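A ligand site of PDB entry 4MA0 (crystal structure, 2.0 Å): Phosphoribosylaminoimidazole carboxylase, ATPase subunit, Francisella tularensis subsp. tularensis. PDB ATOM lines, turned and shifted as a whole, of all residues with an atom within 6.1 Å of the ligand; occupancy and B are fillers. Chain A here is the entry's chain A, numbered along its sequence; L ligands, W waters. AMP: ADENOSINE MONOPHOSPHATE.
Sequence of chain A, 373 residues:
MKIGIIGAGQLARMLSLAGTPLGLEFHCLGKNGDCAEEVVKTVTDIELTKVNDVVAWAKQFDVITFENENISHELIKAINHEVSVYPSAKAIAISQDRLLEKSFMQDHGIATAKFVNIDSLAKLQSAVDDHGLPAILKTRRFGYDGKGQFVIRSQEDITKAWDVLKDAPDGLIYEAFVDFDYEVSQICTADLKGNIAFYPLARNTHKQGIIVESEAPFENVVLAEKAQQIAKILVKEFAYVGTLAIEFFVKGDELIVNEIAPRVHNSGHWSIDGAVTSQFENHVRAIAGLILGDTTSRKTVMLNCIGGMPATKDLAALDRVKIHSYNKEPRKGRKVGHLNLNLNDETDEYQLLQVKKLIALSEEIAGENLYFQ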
ATOM      1  N   ARG A  98       4.222  -3.578 -16.841  1.00  0.00           N
ATOM      2  CA  ARG A  98       4.197  -4.675 -15.868  1.00  0.00           C
ATOM      3  C   ARG A  98       3.040  -5.650 -16.096  1.00  0.00           C
ATOM      4  O   ARG A  98       3.192  -6.843 -15.914  1.00  0.00           O
ATOM      5  CB  ARG A  98       4.158  -4.125 -14.442  1.00  0.00           C
ATOM      6  CG  ARG A  98       5.268  -3.108 -14.164  1.00  0.00           C
ATOM      7  CD  ARG A  98       5.417  -2.872 -12.664  1.00  0.00           C
ATOM      8  NE  ARG A  98       5.794  -4.117 -11.989  1.00  0.00           N
ATOM      9  CZ  ARG A  98       7.050  -4.517 -11.806  1.00  0.00           C
ATOM     10  NH1 ARG A  98       8.060  -3.753 -12.243  1.00  0.00           N
ATOM     11  NH2 ARG A  98       7.302  -5.660 -11.181  1.00  0.00           N
ATOM     12  N   ALA A 113       4.936 -13.279  -9.488  1.00  0.00           N
ATOM     13  CA  ALA A 113       4.077 -12.873  -8.394  1.00  0.00           C
ATOM     14  C   ALA A 113       2.628 -12.955  -8.865  1.00  0.00           C
ATOM     15  O   ALA A 113       2.348 -12.727 -10.051  1.00  0.00           O
ATOM     16  CB  ALA A 113       4.418 -11.446  -7.975  1.00  0.00           C
ATOM     17  N   ILE A 136       1.920  -4.867  -3.130  1.00  0.00           N
ATOM     18  CA  ILE A 136       2.371  -3.612  -3.703  1.00  0.00           C
ATOM     19  C   ILE A 136       1.459  -3.164  -4.836  1.00  0.00           C
ATOM     20  O   ILE A 136       1.074  -3.947  -5.694  1.00  0.00           O
ATOM     21  CB  ILE A 136       3.808  -3.739  -4.241  1.00  0.00           C
ATOM     22  CG1 ILE A 136       4.700  -4.484  -3.238  1.00  0.00           C
ATOM     23  CG2 ILE A 136       4.371  -2.365  -4.571  1.00  0.00           C
ATOM     24  CD1 ILE A 136       6.032  -4.950  -3.807  1.00  0.00           C
ATOM     25  N   LYS A 138       1.619  -0.816  -8.010  1.00  0.00           N
ATOM     26  CA  LYS A 138       2.667  -0.239  -8.855  1.00  0.00           C
ATOM     27  C   LYS A 138       2.082   0.368 -10.114  1.00  0.00           C
ATOM     28  O   LYS A 138       1.078  -0.121 -10.639  1.00  0.00           O
ATOM     29  CB  LYS A 138       3.631  -1.342  -9.304  1.00  0.00           C
ATOM     30  CG  LYS A 138       4.377  -2.063  -8.196  1.00  0.00           C
ATOM     31  CD  LYS A 138       5.438  -2.980  -8.791  1.00  0.00           C
ATOM     32  CE  LYS A 138       6.068  -3.894  -7.740  1.00  0.00           C
ATOM     33  NZ  LYS A 138       6.907  -4.978  -8.342  1.00  0.00           N
ATOM     34  N   GLY A 143       7.873   2.873 -14.032  1.00  0.00           N
ATOM     35  CA  GLY A 143       8.454   2.563 -12.745  1.00  0.00           C
ATOM     36  C   GLY A 143       9.945   2.277 -12.924  1.00  0.00           C
ATOM     37  O   GLY A 143      10.352   1.611 -13.876  1.00  0.00           O
ATOM     38  N   TYR A 144      10.764   2.808 -12.014  1.00  0.00           N
ATOM     39  CA  TYR A 144      12.186   2.442 -11.979  1.00  0.00           C
ATOM     40  C   TYR A 144      12.755   2.745 -10.595  1.00  0.00           C
ATOM     41  O   TYR A 144      12.343   3.717  -9.949  1.00  0.00           O
ATOM     42  CB  TYR A 144      12.987   3.160 -13.087  1.00  0.00           C
ATOM     43  CG  TYR A 144      13.204   4.645 -12.873  1.00  0.00           C
ATOM     44  CD1 TYR A 144      14.318   5.115 -12.169  1.00  0.00           C
ATOM     45  CD2 TYR A 144      12.299   5.586 -13.364  1.00  0.00           C
ATOM     46  CE1 TYR A 144      14.518   6.469 -11.948  1.00  0.00           C
ATOM     47  CE2 TYR A 144      12.494   6.946 -13.162  1.00  0.00           C
ATOM     48  CZ  TYR A 144      13.606   7.380 -12.447  1.00  0.00           C
ATOM     49  OH  TYR A 144      13.804   8.728 -12.238  1.00  0.00           O
ATOM     50  N   ASP A 145      13.693   1.907 -10.147  1.00  0.00           N
ATOM     51  CA  ASP A 145      14.312   2.015  -8.829  1.00  0.00           C
ATOM     52  C   ASP A 145      13.289   1.980  -7.702  1.00  0.00           C
ATOM     53  O   ASP A 145      13.479   2.595  -6.652  1.00  0.00           O
ATOM     54  CB  ASP A 145      15.161   3.275  -8.713  1.00  0.00           C
ATOM     55  CG  ASP A 145      16.419   3.221  -9.545  1.00  0.00           C
ATOM     56  OD1 ASP A 145      16.914   2.101  -9.826  1.00  0.00           O
ATOM     57  OD2 ASP A 145      16.920   4.296  -9.917  1.00  0.00           O
ATOM     58  N   GLY A 146      12.198   1.267  -7.934  1.00  0.00           N
ATOM     59  CA  GLY A 146      11.157   1.113  -6.927  1.00  0.00           C
ATOM     60  C   GLY A 146      10.299   2.341  -6.721  1.00  0.00           C
ATOM     61  O   GLY A 146       9.531   2.408  -5.760  1.00  0.00           O
ATOM     62  N   LYS A 147      10.417   3.315  -7.619  1.00  0.00           N
ATOM     63  CA  LYS A 147       9.586   4.514  -7.539  1.00  0.00           C
ATOM     64  C   LYS A 147       8.272   4.273  -8.254  1.00  0.00           C
ATOM     65  O   LYS A 147       8.164   3.351  -9.065  1.00  0.00           O
ATOM     66  CB  LYS A 147      10.322   5.720  -8.137  1.00  0.00           C
ATOM     67  CG  LYS A 147      11.478   6.217  -7.284  1.00  0.00           C
ATOM     68  CD  LYS A 147      12.307   7.227  -8.026  1.00  0.00           C
ATOM     69  CE  LYS A 147      13.237   7.956  -7.075  1.00  0.00           C
ATOM     70  NZ  LYS A 147      12.458   8.795  -6.110  1.00  0.00           N
ATOM     71  N   GLN A 149       5.421   3.433  -6.730  1.00  0.00           N
ATOM     72  CA  GLN A 149       4.656   2.356  -6.116  1.00  0.00           C
ATOM     73  C   GLN A 149       4.347   2.647  -4.656  1.00  0.00           C
ATOM     74  O   GLN A 149       4.883   3.566  -4.062  1.00  0.00           O
ATOM     75  CB  GLN A 149       5.332   0.991  -6.310  1.00  0.00           C
ATOM     76  CG  GLN A 149       6.807   0.903  -5.986  1.00  0.00           C
ATOM     77  CD  GLN A 149       7.434  -0.337  -6.627  1.00  0.00           C
ATOM     78  OE1 GLN A 149       7.816  -1.282  -5.926  1.00  0.00           O
ATOM     79  NE2 GLN A 149       7.536  -0.341  -7.957  1.00  0.00           N
ATOM     80  N   GLU A 175       0.510  -6.353  -7.006  1.00  0.00           N
ATOM     81  CA  GLU A 175       1.327  -7.539  -6.881  1.00  0.00           C
ATOM     82  C   GLU A 175       1.337  -8.017  -5.442  1.00  0.00           C
ATOM     83  O   GLU A 175       1.528  -7.230  -4.523  1.00  0.00           O
ATOM     84  CB  GLU A 175       2.772  -7.268  -7.308  1.00  0.00           C
ATOM     85  CG  GLU A 175       2.954  -6.893  -8.762  1.00  0.00           C
ATOM     86  CD  GLU A 175       4.414  -6.791  -9.126  1.00  0.00           C
ATOM     87  OE1 GLU A 175       5.260  -7.253  -8.315  1.00  0.00           O
ATOM     88  OE2 GLU A 175       4.722  -6.256 -10.208  1.00  0.00           O
ATOM     89  N   ALA A 176       1.137  -9.313  -5.241  1.00  0.00           N
ATOM     90  CA  ALA A 176       1.254  -9.894  -3.909  1.00  0.00           C
ATOM     91  C   ALA A 176       2.733 -10.083  -3.597  1.00  0.00           C
ATOM     92  O   ALA A 176       3.534 -10.306  -4.497  1.00  0.00           O
ATOM     93  CB  ALA A 176       0.524 -11.216  -3.840  1.00  0.00           C
ATOM     94  N   PHE A 177       3.087 -10.008  -2.318  1.00  0.00           N
ATOM     95  CA  PHE A 177       4.473 -10.232  -1.901  1.00  0.00           C
ATOM     96  C   PHE A 177       4.911 -11.663  -2.218  1.00  0.00           C
ATOM     97  O   PHE A 177       4.181 -12.622  -1.970  1.00  0.00           O
ATOM     98  CB  PHE A 177       4.641  -9.929  -0.407  1.00  0.00           C
ATOM     99  CG  PHE A 177       5.335  -8.625  -0.122  1.00  0.00           C
ATOM    100  CD1 PHE A 177       4.779  -7.422  -0.538  1.00  0.00           C
ATOM    101  CD2 PHE A 177       6.522  -8.608   0.594  1.00  0.00           C
ATOM    102  CE1 PHE A 177       5.419  -6.236  -0.263  1.00  0.00           C
ATOM    103  CE2 PHE A 177       7.159  -7.410   0.863  1.00  0.00           C
ATOM    104  CZ  PHE A 177       6.604  -6.226   0.440  1.00  0.00           C
ATOM    105  N   VAL A 178       6.116 -11.788  -2.762  1.00  0.00           N
ATOM    106  CA  VAL A 178       6.672 -13.097  -3.065  1.00  0.00           C
ATOM    107  C   VAL A 178       7.510 -13.606  -1.896  1.00  0.00           C
ATOM    108  O   VAL A 178       8.305 -12.870  -1.317  1.00  0.00           O
ATOM    109  CB  VAL A 178       7.535 -13.053  -4.325  1.00  0.00           C
ATOM    110  CG1 VAL A 178       8.238 -14.375  -4.547  1.00  0.00           C
ATOM    111  CG2 VAL A 178       6.686 -12.711  -5.533  1.00  0.00           C
ATOM    112  N   ASP A 179       7.287 -14.870  -1.548  1.00  0.00           N
ATOM    113  CA  ASP A 179       8.119 -15.584  -0.593  1.00  0.00           C
ATOM    114  C   ASP A 179       9.394 -16.038  -1.305  1.00  0.00           C
ATOM    115  O   ASP A 179       9.362 -17.015  -2.058  1.00  0.00           O
ATOM    116  CB  ASP A 179       7.355 -16.806  -0.080  1.00  0.00           C
ATOM    117  CG  ASP A 179       8.000 -17.456   1.136  1.00  0.00           C
ATOM    118  OD1 ASP A 179       9.252 -17.547   1.189  1.00  0.00           O
ATOM    119  OD2 ASP A 179       7.253 -17.895   2.031  1.00  0.00           O
ATOM    120  N   PHE A 180      10.501 -15.348  -1.063  1.00  0.00           N
ATOM    121  CA  PHE A 180      11.775 -15.756  -1.662  1.00  0.00           C
ATOM    122  C   PHE A 180      12.967 -15.626  -0.716  1.00  0.00           C
ATOM    123  O   PHE A 180      12.946 -14.867   0.257  1.00  0.00           O
ATOM    124  CB  PHE A 180      12.031 -15.037  -2.987  1.00  0.00           C
ATOM    125  CG  PHE A 180      12.330 -13.574  -2.838  1.00  0.00           C
ATOM    126  CD1 PHE A 180      11.301 -12.650  -2.785  1.00  0.00           C
ATOM    127  CD2 PHE A 180      13.631 -13.131  -2.754  1.00  0.00           C
ATOM    128  CE1 PHE A 180      11.580 -11.307  -2.635  1.00  0.00           C
ATOM    129  CE2 PHE A 180      13.909 -11.787  -2.604  1.00  0.00           C
ATOM    130  CZ  PHE A 180      12.882 -10.882  -2.557  1.00  0.00           C
ATOM    131  N   GLU A 183      17.740 -13.245  -4.738  1.00  0.00           N
ATOM    132  CA  GLU A 183      17.430 -12.862  -6.105  1.00  0.00           C
ATOM    133  C   GLU A 183      18.588 -13.128  -7.028  1.00  0.00           C
ATOM    134  O   GLU A 183      19.746 -12.984  -6.634  1.00  0.00           O
ATOM    135  CB  GLU A 183      17.055 -11.379  -6.173  1.00  0.00           C
ATOM    136  CG  GLU A 183      15.865 -11.037  -5.326  1.00  0.00           C
ATOM    137  CD  GLU A 183      15.479  -9.588  -5.422  1.00  0.00           C
ATOM    138  OE1 GLU A 183      15.033  -9.165  -6.507  1.00  0.00           O
ATOM    139  OE2 GLU A 183      15.639  -8.856  -4.413  1.00  0.00           O
ATOM    140  N   HIS A 206      19.782  -6.083  -3.282  1.00  0.00           N
ATOM    141  CA  HIS A 206      19.092  -4.792  -3.369  1.00  0.00           C
ATOM    142  C   HIS A 206      19.025  -4.089  -2.028  1.00  0.00           C
ATOM    143  O   HIS A 206      19.003  -4.728  -0.967  1.00  0.00           O
ATOM    144  CB  HIS A 206      17.673  -4.964  -3.910  1.00  0.00           C
ATOM    145  CG  HIS A 206      17.633  -5.500  -5.308  1.00  0.00           C
ATOM    146  ND1 HIS A 206      17.605  -6.849  -5.590  1.00  0.00           N
ATOM    147  CD2 HIS A 206      17.611  -4.860  -6.508  1.00  0.00           C
ATOM    148  CE1 HIS A 206      17.562  -7.010  -6.902  1.00  0.00           C
ATOM    149  NE2 HIS A 206      17.576  -5.828  -7.475  1.00  0.00           N
ATOM    150  N   GLY A 209      15.146  -0.869  -2.807  1.00  0.00           N
ATOM    151  CA  GLY A 209      14.645  -1.039  -4.159  1.00  0.00           C
ATOM    152  C   GLY A 209      15.629  -0.777  -5.279  1.00  0.00           C
ATOM    153  O   GLY A 209      15.263  -0.814  -6.456  1.00  0.00           O
ATOM    154  N   GLU A 247      15.303 -10.895 -14.432  1.00  0.00           N
ATOM    155  CA  GLU A 247      15.474 -10.906 -12.983  1.00  0.00           C
ATOM    156  C   GLU A 247      14.472 -11.849 -12.299  1.00  0.00           C
ATOM    157  O   GLU A 247      13.286 -11.801 -12.580  1.00  0.00           O
ATOM    158  CB  GLU A 247      15.307  -9.499 -12.428  1.00  0.00           C
ATOM    159  CG  GLU A 247      16.356  -8.525 -12.942  1.00  0.00           C
ATOM    160  CD  GLU A 247      16.250  -7.183 -12.273  1.00  0.00           C
ATOM    161  OE1 GLU A 247      15.442  -6.353 -12.751  1.00  0.00           O
ATOM    162  OE2 GLU A 247      16.962  -6.971 -11.266  1.00  0.00           O
ATOM    163  N   PHE A 249      13.111 -14.038  -8.582  1.00  0.00           N
ATOM    164  CA  PHE A 249      13.096 -14.350  -7.170  1.00  0.00           C
ATOM    165  C   PHE A 249      13.423 -15.845  -7.049  1.00  0.00           C
ATOM    166  O   PHE A 249      13.002 -16.658  -7.862  1.00  0.00           O
ATOM    167  CB  PHE A 249      11.709 -14.087  -6.583  1.00  0.00           C
ATOM    168  CG  PHE A 249      11.243 -12.670  -6.730  1.00  0.00           C
ATOM    169  CD1 PHE A 249      12.050 -11.613  -6.339  1.00  0.00           C
ATOM    170  CD2 PHE A 249       9.988 -12.396  -7.259  1.00  0.00           C
ATOM    171  CE1 PHE A 249      11.614 -10.300  -6.484  1.00  0.00           C
ATOM    172  CE2 PHE A 249       9.545 -11.088  -7.392  1.00  0.00           C
ATOM    173  CZ  PHE A 249      10.343 -10.042  -7.002  1.00  0.00           C
ATOM    174  N   ASN A 258      10.653 -11.920 -11.900  1.00  0.00           N
ATOM    175  CA  ASN A 258      10.322 -10.618 -11.328  1.00  0.00           C
ATOM    176  C   ASN A 258       9.946  -9.672 -12.468  1.00  0.00           C
ATOM    177  O   ASN A 258       8.806  -9.249 -12.591  1.00  0.00           O
ATOM    178  CB  ASN A 258      11.529 -10.101 -10.550  1.00  0.00           C
ATOM    179  CG  ASN A 258      11.326  -8.690 -10.016  1.00  0.00           C
ATOM    180  OD1 ASN A 258      10.213  -8.232  -9.831  1.00  0.00           O
ATOM    181  ND2 ASN A 258      12.432  -8.010  -9.744  1.00  0.00           N
ATOM    182  N   GLU A 259      10.929  -9.376 -13.315  1.00  0.00           N
ATOM    183  CA  GLU A 259      10.672  -8.581 -14.505  1.00  0.00           C
ATOM    184  C   GLU A 259      11.825  -8.767 -15.477  1.00  0.00           C
ATOM    185  O   GLU A 259      12.848  -9.323 -15.120  1.00  0.00           O
ATOM    186  CB  GLU A 259      10.506  -7.103 -14.157  1.00  0.00           C
ATOM    187  CG  GLU A 259      11.693  -6.483 -13.471  1.00  0.00           C
ATOM    188  CD  GLU A 259      11.575  -4.951 -13.393  1.00  0.00           C
ATOM    189  OE1 GLU A 259      10.447  -4.429 -13.522  1.00  0.00           O
ATOM    190  OE2 GLU A 259      12.605  -4.276 -13.221  1.00  0.00           O
HETATM  191  P   AMP L   1      10.631  -3.061  -9.237  1.00  0.00           P
HETATM  192  O1P AMP L   1      10.995  -4.269 -10.073  1.00  0.00           O
HETATM  193  O2P AMP L   1       9.172  -3.022  -8.851  1.00  0.00           O
HETATM  194  O3P AMP L   1      11.180  -1.734  -9.741  1.00  0.00           O
HETATM  195  O5' AMP L   1      11.345  -3.384  -7.842  1.00  0.00           O
HETATM  196  C5' AMP L   1      12.390  -4.339  -7.768  1.00  0.00           C
HETATM  197  C4' AMP L   1      12.534  -4.935  -6.384  1.00  0.00           C
HETATM  198  O4' AMP L   1      11.311  -4.767  -5.625  1.00  0.00           O
HETATM  199  C3' AMP L   1      12.819  -6.426  -6.347  1.00  0.00           C
HETATM  200  O3' AMP L   1      14.198  -6.716  -6.516  1.00  0.00           O
HETATM  201  C2' AMP L   1      12.260  -6.868  -4.987  1.00  0.00           C
HETATM  202  O2' AMP L   1      13.233  -6.691  -3.960  1.00  0.00           O
HETATM  203  C1' AMP L   1      11.111  -5.880  -4.779  1.00  0.00           C
HETATM  204  N9  AMP L   1       9.804  -6.469  -5.124  1.00  0.00           N
HETATM  205  C8  AMP L   1       9.071  -6.112  -6.187  1.00  0.00           C
HETATM  206  N7  AMP L   1       7.916  -6.823  -6.257  1.00  0.00           N
HETATM  207  C5  AMP L   1       7.915  -7.667  -5.212  1.00  0.00           C
HETATM  208  C6  AMP L   1       6.985  -8.707  -4.689  1.00  0.00           C
HETATM  209  N6  AMP L   1       5.827  -8.966  -5.337  1.00  0.00           N
HETATM  210  N1  AMP L   1       7.348  -9.363  -3.564  1.00  0.00           N
HETATM  211  C2  AMP L   1       8.503  -9.100  -2.926  1.00  0.00           C
HETATM  212  N3  AMP L   1       9.386  -8.176  -3.340  1.00  0.00           N
HETATM  213  C4  AMP L   1       9.157  -7.436  -4.457  1.00  0.00           C
HETATM  214  O   HOH W   1      10.817  -1.805 -12.499  1.00  0.00           O
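OE1 of Glu 259 sits close to O1P of the ligand (3.5 Å).
CB of Ala 113 touches N6 of the ligand, at 3.9 Å.
Ile 136 touches the ligand (CD1 to C5, 3.6 Å).
N of Gly 146 touches O3P of the ligand (3.6 Å).
Phe 177 touches the ligand.
Phe 180 touches the ligand.
CE1 of His 206 touches O3' of the ligand, 3.4 Å away.
CE1 of Phe 249 touches C2' of the ligand (3.8 Å).
Asn 258 touches the ligand (ND2 to C3', 3.8 Å).
16 residues have an atom within 4 Å of the ligand: Arg 98, Ala 113, Ile 136, Lys 138, Gly 146, Gln 149, Glu 175, Ala 176, Phe 177, Val 178, Phe 180, Glu 183, His 206, Phe 249, Asn 258 and Glu 259.
The side-chain carboxylate (OE1) of Glu 259 lies within salt-bridge range of the guanidinium group (NH1) of Arg 98 (2.8 Å).
The backbone NH (N) of Asn 258 is in hydrogen-bond range of the backbone carbonyl oxygen (O) of Glu 247 (2.7 Å).
O of Glu 259 is in hydrogen-bond range of N of Glu 247.
ND1 of His 206 sits at hydrogen-bond distance from OE2 of Glu 183, 3.0 Å away.
N of Ile 136 is in hydrogen-bond range of O of Glu 175 (2.8 Å).
OE2 of Glu 175 is in salt-bridge range of NH2 of Arg 98 (2.8 Å).
OE1 of Glu 175 is in salt-bridge range of NZ of Lys 138 (2.8 Å).
Water W1 lies within hydrogen-bond range of an oxygen (O3P) of the ligand (2.8 Å), the side-chain carboxylate (OE1) of Glu 259 (2.8 Å) and the guanidinium group (NH1) of Arg 98 (3.4 Å).
A nitrogen (N6) of the ligand lies within hydrogen-bond range of the side-chain carboxylate of Glu 175, 3.5 Å away.
O2P of the ligand is in hydrogen-bond range of NE2 of Gln 149, 3.3 Å away.
O of Ala 176 lies within hydrogen-bond range of N6 of the ligand, 2.8 Å away.
The guanidinium group (NH1) of Arg 98 is in salt-bridge range of an oxygen (O2P) of the ligand, 3.6 Å away.
The side-chain carboxylate of Glu 183 is in hydrogen-bond range of an oxygen (O3') of the ligand, 2.6 Å away.
The side-chain amino group of Lys 138 is in salt-bridge range of an oxygen (O2P) of the ligand (3.0 Å).
The backbone NH (N) of Val 178 lies within hydrogen-bond range of a nitrogen (N1) of the ligand.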
